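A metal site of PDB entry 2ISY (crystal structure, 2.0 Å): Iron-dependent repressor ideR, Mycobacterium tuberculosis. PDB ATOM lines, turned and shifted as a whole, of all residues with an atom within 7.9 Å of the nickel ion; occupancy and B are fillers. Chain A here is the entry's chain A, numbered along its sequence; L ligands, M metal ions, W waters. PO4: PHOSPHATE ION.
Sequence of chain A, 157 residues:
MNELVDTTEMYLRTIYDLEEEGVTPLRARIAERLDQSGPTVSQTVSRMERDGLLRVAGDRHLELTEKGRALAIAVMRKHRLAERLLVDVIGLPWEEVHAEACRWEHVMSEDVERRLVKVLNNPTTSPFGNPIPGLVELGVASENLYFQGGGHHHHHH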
ATOM      1  N   ARG A  13     -23.060  -4.225  13.939  1.00  0.00           N
ATOM      2  CA  ARG A  13     -22.315  -5.362  13.376  1.00  0.00           C
ATOM      3  C   ARG A  13     -22.481  -5.444  11.856  1.00  0.00           C
ATOM      4  O   ARG A  13     -21.573  -5.876  11.165  1.00  0.00           O
ATOM      5  CB  ARG A  13     -22.684  -6.731  14.037  1.00  0.00           C
ATOM      6  CG  ARG A  13     -21.426  -7.545  14.539  1.00  0.00           C
ATOM      7  CD  ARG A  13     -21.458  -9.082  14.313  1.00  0.00           C
ATOM      8  NE  ARG A  13     -21.957  -9.377  12.970  1.00  0.00           N
ATOM      9  CZ  ARG A  13     -22.965 -10.204  12.700  1.00  0.00           C
ATOM     10  NH1 ARG A  13     -23.557 -10.922  13.644  1.00  0.00           N
ATOM     11  NH2 ARG A  13     -23.366 -10.328  11.440  1.00  0.00           N
ATOM     12  N   ASP A  17     -19.480  -5.436   9.188  1.00  0.00           N
ATOM     13  CA  ASP A  17     -19.410  -6.462   8.126  1.00  0.00           C
ATOM     14  C   ASP A  17     -19.128  -5.827   6.752  1.00  0.00           C
ATOM     15  O   ASP A  17     -18.228  -6.229   6.012  1.00  0.00           O
ATOM     16  CB  ASP A  17     -20.744  -7.217   8.014  1.00  0.00           C
ATOM     17  CG  ASP A  17     -20.915  -8.255   9.114  1.00  0.00           C
ATOM     18  OD1 ASP A  17     -19.939  -8.538   9.847  1.00  0.00           O
ATOM     19  OD2 ASP A  17     -22.033  -8.798   9.201  1.00  0.00           O
ATOM     20  N   MET A  76     -18.499  -7.878  17.503  1.00  0.00           N
ATOM     21  CA  MET A  76     -17.876  -8.794  16.573  1.00  0.00           C
ATOM     22  C   MET A  76     -16.882  -9.732  17.316  1.00  0.00           C
ATOM     23  O   MET A  76     -16.732 -10.893  16.961  1.00  0.00           O
ATOM     24  CB  MET A  76     -17.153  -8.007  15.451  1.00  0.00           C
ATOM     25  CG  MET A  76     -16.379  -8.926  14.468  1.00  0.00           C
ATOM     26  SD  MET A  76     -17.384 -10.208  13.672  1.00  0.00           S
ATOM     27  CE  MET A  76     -17.933  -9.372  12.208  1.00  0.00           C
ATOM     28  N   HIS A  79     -18.879 -12.300  18.909  1.00  0.00           N
ATOM     29  CA  HIS A  79     -19.392 -13.168  17.857  1.00  0.00           C
ATOM     30  C   HIS A  79     -18.350 -14.257  17.497  1.00  0.00           C
ATOM     31  O   HIS A  79     -18.681 -15.452  17.409  1.00  0.00           O
ATOM     32  CB  HIS A  79     -19.708 -12.335  16.610  1.00  0.00           C
ATOM     33  CG  HIS A  79     -20.235 -13.141  15.475  1.00  0.00           C
ATOM     34  ND1 HIS A  79     -21.530 -13.573  15.407  1.00  0.00           N
ATOM     35  CD2 HIS A  79     -19.632 -13.582  14.341  1.00  0.00           C
ATOM     36  CE1 HIS A  79     -21.726 -14.259  14.301  1.00  0.00           C
ATOM     37  NE2 HIS A  79     -20.589 -14.268  13.633  1.00  0.00           N
ATOM     38  N   ARG A  80     -17.123 -13.840  17.238  1.00  0.00           N
ATOM     39  CA  ARG A  80     -16.089 -14.781  16.810  1.00  0.00           C
ATOM     40  C   ARG A  80     -15.578 -15.706  17.935  1.00  0.00           C
ATOM     41  O   ARG A  80     -15.241 -16.858  17.688  1.00  0.00           O
ATOM     42  CB  ARG A  80     -14.955 -14.034  16.069  1.00  0.00           C
ATOM     43  CG  ARG A  80     -15.429 -13.452  14.707  1.00  0.00           C
ATOM     44  CD  ARG A  80     -14.345 -12.717  13.900  1.00  0.00           C
ATOM     45  NE  ARG A  80     -14.897 -12.474  12.563  1.00  0.00           N
ATOM     46  CZ  ARG A  80     -14.683 -11.409  11.801  1.00  0.00           C
ATOM     47  NH1 ARG A  80     -13.853 -10.422  12.186  1.00  0.00           N
ATOM     48  NH2 ARG A  80     -15.342 -11.334  10.659  1.00  0.00           N
ATOM     49  N   GLU A  83     -18.283 -18.284  18.091  1.00  0.00           N
ATOM     50  CA  GLU A  83     -18.099 -19.274  17.023  1.00  0.00           C
ATOM     51  C   GLU A  83     -16.959 -20.251  17.337  1.00  0.00           C
ATOM     52  O   GLU A  83     -17.098 -21.444  17.114  1.00  0.00           O
ATOM     53  CB  GLU A  83     -17.883 -18.609  15.672  1.00  0.00           C
ATOM     54  CG  GLU A  83     -19.142 -17.941  15.153  1.00  0.00           C
ATOM     55  CD  GLU A  83     -18.862 -17.227  13.852  1.00  0.00           C
ATOM     56  OE1 GLU A  83     -17.731 -16.729  13.698  1.00  0.00           O
ATOM     57  OE2 GLU A  83     -19.783 -17.162  13.009  1.00  0.00           O
ATOM     58  N   VAL A  97     -23.154 -22.843  13.200  1.00  0.00           N
ATOM     59  CA  VAL A  97     -22.485 -22.009  14.219  1.00  0.00           C
ATOM     60  C   VAL A  97     -22.671 -20.490  14.092  1.00  0.00           C
ATOM     61  O   VAL A  97     -22.858 -19.791  15.127  1.00  0.00           O
ATOM     62  CB  VAL A  97     -21.012 -22.449  14.618  1.00  0.00           C
ATOM     63  CG1 VAL A  97     -20.815 -23.985  14.516  1.00  0.00           C
ATOM     64  CG2 VAL A  97     -19.923 -21.674  13.889  1.00  0.00           C
ATOM     65  N   HIS A  98     -22.626 -19.976  12.864  1.00  0.00           N
ATOM     66  CA  HIS A  98     -22.860 -18.520  12.655  1.00  0.00           C
ATOM     67  C   HIS A  98     -24.236 -18.042  13.143  1.00  0.00           C
ATOM     68  O   HIS A  98     -24.341 -17.008  13.832  1.00  0.00           O
ATOM     69  CB  HIS A  98     -22.660 -18.054  11.210  1.00  0.00           C
ATOM     70  CG  HIS A  98     -23.072 -16.621  11.014  1.00  0.00           C
ATOM     71  ND1 HIS A  98     -22.256 -15.562  11.345  1.00  0.00           N
ATOM     72  CD2 HIS A  98     -24.257 -16.082  10.606  1.00  0.00           C
ATOM     73  CE1 HIS A  98     -22.899 -14.428  11.120  1.00  0.00           C
ATOM     74  NE2 HIS A  98     -24.127 -14.718  10.691  1.00  0.00           N
ATOM     75  N   ALA A  99     -25.280 -18.769  12.758  1.00  0.00           N
ATOM     76  CA  ALA A  99     -26.629 -18.468  13.190  1.00  0.00           C
ATOM     77  C   ALA A  99     -26.700 -18.429  14.721  1.00  0.00           C
ATOM     78  O   ALA A  99     -27.332 -17.539  15.289  1.00  0.00           O
ATOM     79  CB  ALA A  99     -27.622 -19.508  12.652  1.00  0.00           C
ATOM     80  N   ALA A 101     -24.161 -18.049  16.956  1.00  0.00           N
ATOM     81  CA  ALA A 101     -23.279 -16.963  17.358  1.00  0.00           C
ATOM     82  C   ALA A 101     -23.921 -15.588  17.137  1.00  0.00           C
ATOM     83  O   ALA A 101     -23.720 -14.645  17.919  1.00  0.00           O
ATOM     84  CB  ALA A 101     -21.994 -17.057  16.573  1.00  0.00           C
ATOM     85  N   CSO A 102     -24.688 -15.476  16.064  1.00  0.00           N
ATOM     86  CA  CSO A 102     -25.467 -14.246  15.814  1.00  0.00           C
ATOM     87  CB  CSO A 102     -26.224 -14.434  14.522  1.00  0.00           C
ATOM     88  SG  CSO A 102     -27.497 -13.212  14.149  1.00  0.00           S
ATOM     89  C   CSO A 102     -26.450 -13.921  16.960  1.00  0.00           C
ATOM     90  O   CSO A 102     -26.805 -12.752  17.159  1.00  0.00           O
ATOM     91  OD  CSO A 102     -26.750 -11.857  14.406  1.00  0.00           O
ATOM     92  N   GLU A 105     -23.823 -13.378  20.482  1.00  0.00           N
ATOM     93  CA  GLU A 105     -22.984 -12.192  20.492  1.00  0.00           C
ATOM     94  C   GLU A 105     -23.610 -11.050  21.276  1.00  0.00           C
ATOM     95  O   GLU A 105     -22.915 -10.169  21.696  1.00  0.00           O
ATOM     96  CB  GLU A 105     -22.721 -11.707  19.061  1.00  0.00           C
ATOM     97  CG  GLU A 105     -23.976 -11.308  18.289  1.00  0.00           C
ATOM     98  CD  GLU A 105     -23.700 -11.048  16.818  1.00  0.00           C
ATOM     99  OE1 GLU A 105     -22.514 -11.067  16.443  1.00  0.00           O
ATOM    100  OE2 GLU A 105     -24.659 -10.780  16.068  1.00  0.00           O
ATOM    101  N   SER A 126     -11.693 -16.403  13.976  1.00  0.00           N
ATOM    102  CA  SER A 126     -12.887 -17.221  14.083  1.00  0.00           C
ATOM    103  C   SER A 126     -12.616 -18.571  13.406  1.00  0.00           C
ATOM    104  O   SER A 126     -11.605 -18.741  12.700  1.00  0.00           O
ATOM    105  CB  SER A 126     -14.054 -16.518  13.412  1.00  0.00           C
ATOM    106  OG  SER A 126     -13.902 -16.529  12.014  1.00  0.00           O
ATOM    107  N   PRO A 127     -13.519 -19.534  13.592  1.00  0.00           N
ATOM    108  CA  PRO A 127     -13.413 -20.817  12.885  1.00  0.00           C
ATOM    109  C   PRO A 127     -13.371 -20.657  11.374  1.00  0.00           C
ATOM    110  O   PRO A 127     -12.939 -21.570  10.686  1.00  0.00           O
ATOM    111  CB  PRO A 127     -14.709 -21.523  13.267  1.00  0.00           C
ATOM    112  CG  PRO A 127     -15.089 -20.928  14.564  1.00  0.00           C
ATOM    113  CD  PRO A 127     -14.705 -19.488  14.464  1.00  0.00           C
ATOM    114  N   PHE A 128     -13.836 -19.528  10.845  1.00  0.00           N
ATOM    115  CA  PHE A 128     -13.964 -19.328   9.396  1.00  0.00           C
ATOM    116  C   PHE A 128     -12.811 -18.520   8.803  1.00  0.00           C
ATOM    117  O   PHE A 128     -12.878 -18.076   7.650  1.00  0.00           O
ATOM    118  CB  PHE A 128     -15.285 -18.627   9.084  1.00  0.00           C
ATOM    119  CG  PHE A 128     -16.499 -19.396   9.564  1.00  0.00           C
ATOM    120  CD1 PHE A 128     -17.103 -19.073  10.767  1.00  0.00           C
ATOM    121  CD2 PHE A 128     -17.004 -20.445   8.829  1.00  0.00           C
ATOM    122  CE1 PHE A 128     -18.206 -19.776  11.221  1.00  0.00           C
ATOM    123  CE2 PHE A 128     -18.120 -21.161   9.270  1.00  0.00           C
ATOM    124  CZ  PHE A 128     -18.716 -20.815  10.473  1.00  0.00           C
ATOM    125  N   ASN A 130     -11.373 -15.555   9.954  1.00  0.00           N
ATOM    126  CA  ASN A 130     -11.359 -14.100  10.053  1.00  0.00           C
ATOM    127  C   ASN A 130     -10.789 -13.657  11.376  1.00  0.00           C
ATOM    128  O   ASN A 130     -11.043 -14.287  12.398  1.00  0.00           O
ATOM    129  CB  ASN A 130     -12.775 -13.559   9.856  1.00  0.00           C
ATOM    130  CG  ASN A 130     -13.329 -13.901   8.482  1.00  0.00           C
ATOM    131  OD1 ASN A 130     -12.752 -13.540   7.477  1.00  0.00           O
ATOM    132  ND2 ASN A 130     -14.462 -14.609   8.434  1.00  0.00           N
HETATM  133  P   PO4 L   1     -17.096 -14.798  10.674  1.00  0.00           P
HETATM  134  O1  PO4 L   1     -17.360 -15.796   9.557  1.00  0.00           O
HETATM  135  O2  PO4 L   1     -15.667 -14.856  11.133  1.00  0.00           O
HETATM  136  O3  PO4 L   1     -17.489 -13.410  10.248  1.00  0.00           O
HETATM  137  O4  PO4 L   1     -18.009 -15.143  11.853  1.00  0.00           O
HETATM  138 NI    NI M   1     -20.157 -15.437  11.789  1.00  0.00          NI
HETATM  139  O   HOH W   1     -20.058 -13.510  10.419  1.00  0.00           O
HETATM  140  O   HOH W   2     -19.742 -16.626  10.003  1.00  0.00           O
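The side-chain carboxylate (OE1) of Glu 105 sits at hydrogen-bond distance from a ring nitrogen (ND1) of His 79 (2.9 Å).
Of the 16 residues printed, 3 come within 4 Å of the nickel ion. The nearest printed residue that does not touch the nickel ion is Phe 128 (4.8 Å).
The nickel ion is bound by OE2 of Glu 83 (2.1 Å). ND1 of His 98 is bound to the nickel ion (2.1 Å). An oxygen (O4) of the ligand is bound to the nickel ion, 2.2 Å away. Water W2 is bound to the nickel ion (2.2 Å). A ring nitrogen (NE2) of His 79 binds the nickel ion, 2.2 Å away. The nickel ion is bound by water W1, 2.4 Å away.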
